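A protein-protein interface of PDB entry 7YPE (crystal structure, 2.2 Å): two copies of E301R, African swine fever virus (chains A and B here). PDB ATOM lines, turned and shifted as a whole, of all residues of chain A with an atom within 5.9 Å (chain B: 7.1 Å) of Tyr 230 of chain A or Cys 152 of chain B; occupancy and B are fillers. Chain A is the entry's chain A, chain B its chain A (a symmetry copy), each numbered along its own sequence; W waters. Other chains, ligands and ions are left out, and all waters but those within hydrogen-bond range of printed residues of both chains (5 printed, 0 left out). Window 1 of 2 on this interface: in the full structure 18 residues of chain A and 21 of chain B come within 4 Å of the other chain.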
ATOM      1  N   THR A 196       5.478 -16.195 -34.829  1.00  0.00           N
ATOM      2  CA  THR A 196       5.829 -16.000 -33.425  1.00  0.00           C
ATOM      3  C   THR A 196       6.699 -14.765 -33.237  1.00  0.00           C
ATOM      4  O   THR A 196       6.405 -13.905 -32.399  1.00  0.00           O
ATOM      5  CB  THR A 196       6.543 -17.243 -32.888  1.00  0.00           C
ATOM      6  OG1 THR A 196       5.603 -18.316 -32.751  1.00  0.00           O
ATOM      7  CG2 THR A 196       7.191 -16.951 -31.541  1.00  0.00           C
ATOM      8  N   ASP A 199       5.031 -11.301 -34.403  1.00  0.00           N
ATOM      9  CA  ASP A 199       4.097 -10.820 -33.390  1.00  0.00           C
ATOM     10  C   ASP A 199       4.834 -10.349 -32.145  1.00  0.00           C
ATOM     11  O   ASP A 199       4.437  -9.362 -31.514  1.00  0.00           O
ATOM     12  CB  ASP A 199       3.096 -11.917 -33.032  1.00  0.00           C
ATOM     13  CG  ASP A 199       2.173 -12.266 -34.183  1.00  0.00           C
ATOM     14  OD1 ASP A 199       2.284 -11.631 -35.252  1.00  0.00           O
ATOM     15  OD2 ASP A 199       1.336 -13.178 -34.016  1.00  0.00           O
ATOM     16  N   LEU A 200       5.911 -11.045 -31.773  1.00  0.00           N
ATOM     17  CA  LEU A 200       6.713 -10.616 -30.632  1.00  0.00           C
ATOM     18  C   LEU A 200       7.371  -9.270 -30.903  1.00  0.00           C
ATOM     19  O   LEU A 200       7.420  -8.405 -30.021  1.00  0.00           O
ATOM     20  CB  LEU A 200       7.768 -11.672 -30.307  1.00  0.00           C
ATOM     21  CG  LEU A 200       7.305 -12.893 -29.507  1.00  0.00           C
ATOM     22  CD1 LEU A 200       8.411 -13.935 -29.441  1.00  0.00           C
ATOM     23  CD2 LEU A 200       6.857 -12.490 -28.110  1.00  0.00           C
ATOM     24  N   LEU A 220       6.616 -19.126 -24.011  1.00  0.00           N
ATOM     25  CA  LEU A 220       7.257 -17.923 -24.528  1.00  0.00           C
ATOM     26  C   LEU A 220       6.439 -16.724 -24.073  1.00  0.00           C
ATOM     27  O   LEU A 220       5.226 -16.681 -24.298  1.00  0.00           O
ATOM     28  CB  LEU A 220       7.347 -17.940 -26.058  1.00  0.00           C
ATOM     29  CG  LEU A 220       8.543 -18.599 -26.748  1.00  0.00           C
ATOM     30  CD1 LEU A 220       8.649 -20.074 -26.394  1.00  0.00           C
ATOM     31  CD2 LEU A 220       8.456 -18.411 -28.256  1.00  0.00           C
ATOM     32  N   TYR A 221       7.092 -15.755 -23.435  1.00  0.00           N
ATOM     33  CA  TYR A 221       6.338 -14.647 -22.866  1.00  0.00           C
ATOM     34  C   TYR A 221       7.241 -13.448 -22.622  1.00  0.00           C
ATOM     35  O   TYR A 221       8.466 -13.565 -22.532  1.00  0.00           O
ATOM     36  CB  TYR A 221       5.643 -15.059 -21.561  1.00  0.00           C
ATOM     37  CG  TYR A 221       6.585 -15.414 -20.426  1.00  0.00           C
ATOM     38  CD1 TYR A 221       7.080 -16.706 -20.287  1.00  0.00           C
ATOM     39  CD2 TYR A 221       6.962 -14.464 -19.485  1.00  0.00           C
ATOM     40  CE1 TYR A 221       7.935 -17.037 -19.248  1.00  0.00           C
ATOM     41  CE2 TYR A 221       7.814 -14.786 -18.445  1.00  0.00           C
ATOM     42  CZ  TYR A 221       8.299 -16.074 -18.331  1.00  0.00           C
ATOM     43  OH  TYR A 221       9.145 -16.399 -17.296  1.00  0.00           O
ATOM     44  N   PHE A 222       6.599 -12.284 -22.534  1.00  0.00           N
ATOM     45  CA  PHE A 222       7.198 -11.073 -21.995  1.00  0.00           C
ATOM     46  C   PHE A 222       6.143 -10.371 -21.153  1.00  0.00           C
ATOM     47  O   PHE A 222       4.942 -10.618 -21.300  1.00  0.00           O
ATOM     48  CB  PHE A 222       7.724 -10.142 -23.099  1.00  0.00           C
ATOM     49  CG  PHE A 222       6.646  -9.553 -23.968  1.00  0.00           C
ATOM     50  CD1 PHE A 222       5.970  -8.405 -23.584  1.00  0.00           C
ATOM     51  CD2 PHE A 222       6.317 -10.146 -25.173  1.00  0.00           C
ATOM     52  CE1 PHE A 222       4.980  -7.869 -24.380  1.00  0.00           C
ATOM     53  CE2 PHE A 222       5.335  -9.610 -25.976  1.00  0.00           C
ATOM     54  CZ  PHE A 222       4.662  -8.474 -25.576  1.00  0.00           C
ATOM     55  N   GLN A 223       6.595  -9.485 -20.271  1.00  0.00           N
ATOM     56  CA  GLN A 223       5.701  -8.781 -19.363  1.00  0.00           C
ATOM     57  C   GLN A 223       6.048  -7.301 -19.333  1.00  0.00           C
ATOM     58  O   GLN A 223       7.213  -6.934 -19.153  1.00  0.00           O
ATOM     59  CB  GLN A 223       5.771  -9.370 -17.951  1.00  0.00           C
ATOM     60  CG  GLN A 223       5.042 -10.696 -17.802  1.00  0.00           C
ATOM     61  CD  GLN A 223       4.986 -11.172 -16.365  1.00  0.00           C
ATOM     62  OE1 GLN A 223       6.017 -11.343 -15.715  1.00  0.00           O
ATOM     63  NE2 GLN A 223       3.777 -11.391 -15.860  1.00  0.00           N
ATOM     64  N   ILE A 228       0.769  -4.156 -21.370  1.00  0.00           N
ATOM     65  CA  ILE A 228       0.540  -5.415 -21.996  1.00  0.00           C
ATOM     66  C   ILE A 228       1.505  -6.518 -21.663  1.00  0.00           C
ATOM     67  O   ILE A 228       2.678  -6.340 -21.694  1.00  0.00           O
ATOM     68  CB  ILE A 228       0.500  -5.246 -23.522  1.00  0.00           C
ATOM     69  CG1 ILE A 228       0.388  -6.574 -24.208  1.00  0.00           C
ATOM     70  CG2 ILE A 228       1.718  -4.523 -24.010  1.00  0.00           C
ATOM     71  CD1 ILE A 228       0.468  -6.497 -25.702  1.00  0.00           C
ATOM     72  N   SER A 229       0.954  -7.653 -21.321  1.00  0.00           N
ATOM     73  CA  SER A 229       1.742  -8.865 -21.166  1.00  0.00           C
ATOM     74  C   SER A 229       1.262  -9.886 -22.187  1.00  0.00           C
ATOM     75  O   SER A 229       0.062  -9.982 -22.464  1.00  0.00           O
ATOM     76  CB  SER A 229       1.626  -9.436 -19.750  1.00  0.00           C
ATOM     77  OG  SER A 229       2.216  -8.567 -18.799  1.00  0.00           O
ATOM     78  N   TYR A 230       2.200 -10.635 -22.754  1.00  0.00           N
ATOM     79  CA  TYR A 230       1.891 -11.593 -23.802  1.00  0.00           C
ATOM     80  C   TYR A 230       2.495 -12.940 -23.452  1.00  0.00           C
ATOM     81  O   TYR A 230       3.650 -13.023 -23.024  1.00  0.00           O
ATOM     82  CB  TYR A 230       2.416 -11.121 -25.157  1.00  0.00           C
ATOM     83  CG  TYR A 230       2.270 -12.130 -26.273  1.00  0.00           C
ATOM     84  CD1 TYR A 230       1.022 -12.443 -26.794  1.00  0.00           C
ATOM     85  CD2 TYR A 230       3.383 -12.762 -26.813  1.00  0.00           C
ATOM     86  CE1 TYR A 230       0.886 -13.360 -27.819  1.00  0.00           C
ATOM     87  CE2 TYR A 230       3.256 -13.680 -27.839  1.00  0.00           C
ATOM     88  CZ  TYR A 230       2.003 -13.975 -28.339  1.00  0.00           C
ATOM     89  OH  TYR A 230       1.869 -14.888 -29.360  1.00  0.00           O
ATOM     90  N   HIS A 231       1.708 -13.994 -23.639  1.00  0.00           N
ATOM     91  CA  HIS A 231       2.136 -15.345 -23.313  1.00  0.00           C
ATOM     92  C   HIS A 231       1.630 -16.281 -24.395  1.00  0.00           C
ATOM     93  O   HIS A 231       0.419 -16.378 -24.615  1.00  0.00           O
ATOM     94  CB  HIS A 231       1.613 -15.770 -21.939  1.00  0.00           C
ATOM     95  CG  HIS A 231       1.804 -17.224 -21.646  1.00  0.00           C
ATOM     96  ND1 HIS A 231       0.906 -17.957 -20.901  1.00  0.00           N
ATOM     97  CD2 HIS A 231       2.788 -18.082 -22.002  1.00  0.00           C
ATOM     98  CE1 HIS A 231       1.331 -19.204 -20.809  1.00  0.00           C
ATOM     99  NE2 HIS A 231       2.468 -19.306 -21.471  1.00  0.00           N
ATOM    100  N   GLU A 232       2.545 -16.963 -25.074  1.00  0.00           N
ATOM    101  CA  GLU A 232       2.169 -17.975 -26.047  1.00  0.00           C
ATOM    102  C   GLU A 232       2.665 -19.326 -25.550  1.00  0.00           C
ATOM    103  O   GLU A 232       3.832 -19.471 -25.169  1.00  0.00           O
ATOM    104  CB  GLU A 232       2.682 -17.623 -27.451  1.00  0.00           C
ATOM    105  CG  GLU A 232       3.999 -18.204 -27.893  1.00  0.00           C
ATOM    106  CD  GLU A 232       4.293 -17.867 -29.345  1.00  0.00           C
ATOM    107  OE1 GLU A 232       3.843 -16.798 -29.812  1.00  0.00           O
ATOM    108  OE2 GLU A 232       4.946 -18.681 -30.029  1.00  0.00           O
ATOM    109  N   MET A 233       1.755 -20.293 -25.509  1.00  0.00           N
ATOM    110  CA  MET A 233       1.992 -21.558 -24.829  1.00  0.00           C
ATOM    111  C   MET A 233       1.670 -22.730 -25.742  1.00  0.00           C
ATOM    112  O   MET A 233       0.632 -22.750 -26.406  1.00  0.00           O
ATOM    113  CB  MET A 233       1.155 -21.625 -23.549  1.00  0.00           C
ATOM    114  CG  MET A 233       1.126 -22.982 -22.869  1.00  0.00           C
ATOM    115  SD  MET A 233       0.053 -22.960 -21.236  1.00  0.00           S
ATOM    116  CE  MET A 233      -1.658 -22.422 -22.004  1.00  0.00           C
ATOM    117  N   MET B 116      -1.953  -6.228 -31.756  1.00  0.00           N
ATOM    118  CA  MET B 116      -2.511  -7.501 -31.309  1.00  0.00           C
ATOM    119  C   MET B 116      -3.640  -7.959 -32.226  1.00  0.00           C
ATOM    120  O   MET B 116      -3.670  -9.111 -32.661  1.00  0.00           O
ATOM    121  CB  MET B 116      -3.021  -7.397 -29.873  1.00  0.00           C
ATOM    122  CG  MET B 116      -3.930  -8.552 -29.469  1.00  0.00           C
ATOM    123  SD  MET B 116      -4.814  -8.274 -27.754  1.00  0.00           S
ATOM    124  CE  MET B 116      -6.493  -7.544 -28.408  1.00  0.00           C
ATOM    125  N   SER B 119      -2.442  -9.019 -35.568  1.00  0.00           N
ATOM    126  CA  SER B 119      -1.784 -10.318 -35.587  1.00  0.00           C
ATOM    127  C   SER B 119      -2.745 -11.463 -35.870  1.00  0.00           C
ATOM    128  O   SER B 119      -2.289 -12.595 -36.064  1.00  0.00           O
ATOM    129  CB  SER B 119      -1.073 -10.563 -34.257  1.00  0.00           C
ATOM    130  OG  SER B 119      -1.983 -11.062 -33.290  1.00  0.00           O
ATOM    131  N   PHE B 124      -5.398 -18.793 -36.538  1.00  0.00           N
ATOM    132  CA  PHE B 124      -6.209 -18.743 -35.328  1.00  0.00           C
ATOM    133  C   PHE B 124      -7.653 -19.065 -35.687  1.00  0.00           C
ATOM    134  O   PHE B 124      -8.276 -18.342 -36.474  1.00  0.00           O
ATOM    135  CB  PHE B 124      -6.124 -17.368 -34.662  1.00  0.00           C
ATOM    136  CG  PHE B 124      -4.774 -17.048 -34.088  1.00  0.00           C
ATOM    137  CD1 PHE B 124      -4.008 -18.034 -33.483  1.00  0.00           C
ATOM    138  CD2 PHE B 124      -4.274 -15.757 -34.144  1.00  0.00           C
ATOM    139  CE1 PHE B 124      -2.767 -17.736 -32.949  1.00  0.00           C
ATOM    140  CE2 PHE B 124      -3.034 -15.453 -33.612  1.00  0.00           C
ATOM    141  CZ  PHE B 124      -2.279 -16.445 -33.014  1.00  0.00           C
ATOM    142  N   THR B 128     -10.849 -15.719 -27.686  1.00  0.00           N
ATOM    143  CA  THR B 128     -11.470 -15.783 -26.372  1.00  0.00           C
ATOM    144  C   THR B 128     -11.182 -14.487 -25.629  1.00  0.00           C
ATOM    145  O   THR B 128     -10.044 -14.006 -25.634  1.00  0.00           O
ATOM    146  CB  THR B 128     -10.959 -16.990 -25.573  1.00  0.00           C
ATOM    147  OG1 THR B 128     -11.202 -18.190 -26.317  1.00  0.00           O
ATOM    148  CG2 THR B 128     -11.668 -17.088 -24.227  1.00  0.00           C
ATOM    149  N   PHE B 141      -7.167 -11.565 -23.846  1.00  0.00           N
ATOM    150  CA  PHE B 141      -7.455 -11.963 -25.220  1.00  0.00           C
ATOM    151  C   PHE B 141      -6.636 -13.209 -25.529  1.00  0.00           C
ATOM    152  O   PHE B 141      -5.405 -13.181 -25.437  1.00  0.00           O
ATOM    153  CB  PHE B 141      -7.122 -10.846 -26.211  1.00  0.00           C
ATOM    154  CG  PHE B 141      -7.977  -9.620 -26.061  1.00  0.00           C
ATOM    155  CD1 PHE B 141      -7.639  -8.629 -25.153  1.00  0.00           C
ATOM    156  CD2 PHE B 141      -9.113  -9.453 -26.836  1.00  0.00           C
ATOM    157  CE1 PHE B 141      -8.422  -7.496 -25.016  1.00  0.00           C
ATOM    158  CE2 PHE B 141      -9.902  -8.324 -26.703  1.00  0.00           C
ATOM    159  CZ  PHE B 141      -9.553  -7.343 -25.793  1.00  0.00           C
ATOM    160  N   ILE B 142      -7.315 -14.294 -25.893  1.00  0.00           N
ATOM    161  CA  ILE B 142      -6.671 -15.577 -26.150  1.00  0.00           C
ATOM    162  C   ILE B 142      -6.973 -15.995 -27.581  1.00  0.00           C
ATOM    163  O   ILE B 142      -8.142 -16.137 -27.961  1.00  0.00           O
ATOM    164  CB  ILE B 142      -7.129 -16.657 -25.156  1.00  0.00           C
ATOM    165  CG1 ILE B 142      -6.830 -16.224 -23.720  1.00  0.00           C
ATOM    166  CG2 ILE B 142      -6.448 -17.981 -25.461  1.00  0.00           C
ATOM    167  CD1 ILE B 142      -8.011 -16.345 -22.785  1.00  0.00           C
ATOM    168  N   PHE B 143      -5.921 -16.189 -28.372  1.00  0.00           N
ATOM    169  CA  PHE B 143      -6.027 -16.709 -29.729  1.00  0.00           C
ATOM    170  C   PHE B 143      -5.439 -18.112 -29.761  1.00  0.00           C
ATOM    171  O   PHE B 143      -4.336 -18.339 -29.252  1.00  0.00           O
ATOM    172  CB  PHE B 143      -5.304 -15.799 -30.724  1.00  0.00           C
ATOM    173  CG  PHE B 143      -5.726 -14.358 -30.645  1.00  0.00           C
ATOM    174  CD1 PHE B 143      -7.009 -13.979 -31.002  1.00  0.00           C
ATOM    175  CD2 PHE B 143      -4.840 -13.385 -30.212  1.00  0.00           C
ATOM    176  CE1 PHE B 143      -7.402 -12.655 -30.927  1.00  0.00           C
ATOM    177  CE2 PHE B 143      -5.227 -12.059 -30.137  1.00  0.00           C
ATOM    178  CZ  PHE B 143      -6.511 -11.694 -30.495  1.00  0.00           C
ATOM    179  N   THR B 144      -6.170 -19.051 -30.357  1.00  0.00           N
ATOM    180  CA  THR B 144      -5.805 -20.461 -30.320  1.00  0.00           C
ATOM    181  C   THR B 144      -5.472 -20.958 -31.719  1.00  0.00           C
ATOM    182  O   THR B 144      -6.263 -20.787 -32.651  1.00  0.00           O
ATOM    183  CB  THR B 144      -6.932 -21.302 -29.715  1.00  0.00           C
ATOM    184  OG1 THR B 144      -7.261 -20.795 -28.416  1.00  0.00           O
ATOM    185  CG2 THR B 144      -6.501 -22.755 -29.588  1.00  0.00           C
ATOM    186  N   ASP B 145      -4.297 -21.570 -31.855  1.00  0.00           N
ATOM    187  CA  ASP B 145      -3.879 -22.249 -33.076  1.00  0.00           C
ATOM    188  C   ASP B 145      -4.041 -23.747 -32.839  1.00  0.00           C
ATOM    189  O   ASP B 145      -3.259 -24.352 -32.098  1.00  0.00           O
ATOM    190  CB  ASP B 145      -2.434 -21.889 -33.426  1.00  0.00           C
ATOM    191  CG  ASP B 145      -1.956 -22.522 -34.731  1.00  0.00           C
ATOM    192  OD1 ASP B 145      -2.551 -23.520 -35.192  1.00  0.00           O
ATOM    193  OD2 ASP B 145      -0.964 -22.017 -35.295  1.00  0.00           O
ATOM    194  N   LYS B 150      -1.337 -24.221 -29.951  1.00  0.00           N
ATOM    195  CA  LYS B 150      -0.630 -23.050 -29.454  1.00  0.00           C
ATOM    196  C   LYS B 150      -1.651 -22.022 -28.985  1.00  0.00           C
ATOM    197  O   LYS B 150      -2.529 -21.615 -29.756  1.00  0.00           O
ATOM    198  CB  LYS B 150       0.279 -22.458 -30.531  1.00  0.00           C
ATOM    199  CG  LYS B 150       0.642 -21.002 -30.297  1.00  0.00           C
ATOM    200  CD  LYS B 150       1.621 -20.503 -31.344  1.00  0.00           C
ATOM    201  CE  LYS B 150       0.907 -19.756 -32.455  1.00  0.00           C
ATOM    202  NZ  LYS B 150       1.859 -19.241 -33.477  1.00  0.00           N
ATOM    203  N   GLU B 151      -1.538 -21.610 -27.726  1.00  0.00           N
ATOM    204  CA  GLU B 151      -2.436 -20.637 -27.119  1.00  0.00           C
ATOM    205  C   GLU B 151      -1.679 -19.333 -26.912  1.00  0.00           C
ATOM    206  O   GLU B 151      -0.682 -19.302 -26.183  1.00  0.00           O
ATOM    207  CB  GLU B 151      -2.981 -21.158 -25.789  1.00  0.00           C
ATOM    208  CG  GLU B 151      -4.490 -21.112 -25.668  1.00  0.00           C
ATOM    209  CD  GLU B 151      -4.989 -21.827 -24.429  1.00  0.00           C
ATOM    210  OE1 GLU B 151      -4.651 -21.382 -23.312  1.00  0.00           O
ATOM    211  OE2 GLU B 151      -5.718 -22.832 -24.573  1.00  0.00           O
ATOM    212  N   CYS B 152      -2.152 -18.264 -27.550  1.00  0.00           N
ATOM    213  CA  CYS B 152      -1.537 -16.943 -27.454  1.00  0.00           C
ATOM    214  C   CYS B 152      -2.427 -16.063 -26.586  1.00  0.00           C
ATOM    215  O   CYS B 152      -3.530 -15.688 -26.998  1.00  0.00           O
ATOM    216  CB  CYS B 152      -1.335 -16.333 -28.840  1.00  0.00           C
ATOM    217  SG  CYS B 152      -0.359 -17.363 -29.964  1.00  0.00           S
ATOM    218  N   THR B 153      -1.943 -15.731 -25.394  1.00  0.00           N
ATOM    219  CA  THR B 153      -2.718 -14.995 -24.401  1.00  0.00           C
ATOM    220  C   THR B 153      -2.167 -13.582 -24.277  1.00  0.00           C
ATOM    221  O   THR B 153      -0.973 -13.397 -24.014  1.00  0.00           O
ATOM    222  CB  THR B 153      -2.682 -15.701 -23.045  1.00  0.00           C
ATOM    223  OG1 THR B 153      -3.229 -17.019 -23.179  1.00  0.00           O
ATOM    224  CG2 THR B 153      -3.491 -14.925 -22.017  1.00  0.00           C
ATOM    225  N   TYR B 154      -3.037 -12.595 -24.470  1.00  0.00           N
ATOM    226  CA  TYR B 154      -2.702 -11.191 -24.281  1.00  0.00           C
ATOM    227  C   TYR B 154      -3.339 -10.700 -22.989  1.00  0.00           C
ATOM    228  O   TYR B 154      -4.534 -10.915 -22.759  1.00  0.00           O
ATOM    229  CB  TYR B 154      -3.189 -10.340 -25.454  1.00  0.00           C
ATOM    230  CG  TYR B 154      -2.406 -10.519 -26.735  1.00  0.00           C
ATOM    231  CD1 TYR B 154      -2.659 -11.590 -27.582  1.00  0.00           C
ATOM    232  CD2 TYR B 154      -1.423  -9.610 -27.103  1.00  0.00           C
ATOM    233  CE1 TYR B 154      -1.950 -11.754 -28.758  1.00  0.00           C
ATOM    234  CE2 TYR B 154      -0.707  -9.766 -28.275  1.00  0.00           C
ATOM    235  CZ  TYR B 154      -0.975 -10.840 -29.099  1.00  0.00           C
ATOM    236  OH  TYR B 154      -0.263 -11.000 -30.266  1.00  0.00           O
ATOM    237  N   GLN B 155      -2.541 -10.047 -22.152  1.00  0.00           N
ATOM    238  CA  GLN B 155      -3.021  -9.389 -20.939  1.00  0.00           C
ATOM    239  C   GLN B 155      -3.008  -7.890 -21.210  1.00  0.00           C
ATOM    240  O   GLN B 155      -1.945  -7.264 -21.227  1.00  0.00           O
ATOM    241  CB  GLN B 155      -2.155  -9.748 -19.737  1.00  0.00           C
ATOM    242  CG  GLN B 155      -2.712 -10.874 -18.888  1.00  0.00           C
ATOM    243  CD  GLN B 155      -1.786 -11.264 -17.754  1.00  0.00           C
ATOM    244  OE1 GLN B 155      -1.671 -10.551 -16.758  1.00  0.00           O
ATOM    245  NE2 GLN B 155      -1.122 -12.406 -17.899  1.00  0.00           N
HETATM  246  O   HOH W   1       4.194 -20.490 -33.735  1.00  0.00           O
HETATM  247  O   HOH W   2      -0.956 -13.142 -31.518  1.00  0.00           O
HETATM  248  O   HOH W   3      -1.284 -18.623 -23.535  1.00  0.00           O
HETATM  249  O   HOH W   4       1.400  -8.973 -31.551  1.00  0.00           O
HETATM  250  O   HOH W   5       2.357 -16.760 -32.570  1.00  0.00           O
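Water W3 lies within hydrogen-bond range of the side-chain hydroxyl of Thr 153 of chain B (2.5 Å), the backbone carbonyl oxygen of Glu 151 of chain B (2.8 Å) and the backbone carbonyl oxygen of His 231 of chain A (3.0 Å). Water W2 lies within hydrogen-bond range of the side-chain hydroxyl (OH) of Tyr 154 of chain B (2.6 Å), the side-chain hydroxyl (OG) of Ser 119 of chain B (2.9 Å) and the side-chain carboxylate (OD2) of Asp 199 of chain A (3.4 Å). Water W1 lies within hydrogen-bond range of the side-chain amino group (NZ) of Lys 150 of chain B and the side-chain hydroxyl (OG1) of Thr 196 of chain A. Water W5 bridges NZ of Lys 150 of chain B and OE1 of Glu 232 of chain A. Water W4 lies within hydrogen-bond range of OH of Tyr 154 of chain B (2.9 Å) and O of Asp 199 of chain A (3.1 Å).
The backbone carbonyl oxygen (O) of Tyr 230 of chain A is in hydrogen-bond range of the backbone NH (N) of Phe 222 of chain A, 3.1 Å away. OE2 of Glu 232 of chain A sits at hydrogen-bond distance from OG1 of Thr 196 of chain A. The backbone carbonyl oxygen (O) of Leu 220 of chain A lies within hydrogen-bond range of the backbone NH (N) of Glu 232 of chain A. The backbone NH (N) of Cys 152 of chain B sits at hydrogen-bond distance from the backbone carbonyl oxygen (O) of Phe 143 of chain B. OE1 of Glu 232 of chain A sits at hydrogen-bond distance from OH of Tyr 230 of chain A. The backbone NH (N) of Asp 145 of chain B is in hydrogen-bond range of the backbone carbonyl oxygen (O) of Lys 150 of chain B (2.7 Å).
N of Met 233 of chain A is in hydrogen-bond range of O of Glu 151 of chain B, 2.7 Å away. The backbone carbonyl oxygen (O) of Ser 229 of chain A lies within hydrogen-bond range of the backbone NH (N) of Gln 155 of chain B, at 2.6 Å. The backbone carbonyl oxygen (O) of His 231 of chain A sits at hydrogen-bond distance from the backbone NH (N) of Thr 153 of chain B, 2.6 Å away. O of His 231 of chain A sits close to O of Glu 151 of chain B (3.5 Å). The side-chain hydroxyl (OH) of Tyr 230 of chain A is in hydrogen-bond range of the side-chain sulfur (SG) of Cys 152 of chain B (3.4 Å).
Of the 15 printed residues of chain B, 7 touch a printed residue of chain A. Printed residues of chain B that touch a printed residue of chain A: Ser 119, Lys 150, Glu 151, Cys 152, Thr 153, Tyr 154 and Gln 155. Hydrophobic or aromatic side chains of chain B within 4 Å of the printed part of chain A: Tyr 154. Printed residues of chain A that touch a printed residue of chain B: Thr 196, Asp 199, Ile 228, Ser 229, Tyr 230, His 231, Glu 232 and Met 233. Hydrophobic or aromatic side chains of chain A that line the printed part of chain B: Ile 228, Tyr 230 and Met 233.
No position is printed for both chains. Of the 17 pairs that touch across the chains among the printed residues, none has its exchanged pair printed and touching as well.
Printed residues of chain B within 4 Å of Thr 196 of chain A: Lys 150. Of the printed residues of chain B, Asp 199 of chain A touches Ser 119. Of the printed residues of chain B, Ile 228 of chain A touches Tyr 154 (3.9 Å) and Gln 155 (3.2 Å). Printed residues of chain B within 4 Å of His 231 of chain A: Glu 151, Cys 152 and Thr 153. Met 116 of chain B touches none of the printed residues of chain A. Cys 152 of chain B touches just these residues of chain A: Tyr 230, His 231 and Glu 232. Printed residues of chain A within 4 Å of Thr 153 of chain B: Ser 229, Tyr 230 and His 231.
Lys 150 of chain B touches Thr 196 of chain A. Ser 119 of chain B touches Asp 199 of chain A (CB to OD2, 3.6 Å). Ile 228 of chain A touches Tyr 154 of chain B (CD1 to CD2, 3.9 Å). Ile 228 of chain A touches Gln 155 of chain B (CA to O, 3.2 Å). Ser 229 of chain A touches Thr 153 of chain B (O to O, 3.9 Å). Ser 229 of chain A touches Tyr 154 of chain B (O to C, 3.5 Å). Tyr 230 of chain A touches Thr 153 of chain B. Cys 152 of chain B touches His 231 of chain A. Glu 151 of chain B touches Glu 232 of chain A (O to CA, 3.1 Å). Met 233 of chain A touches Lys 150 of chain B.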
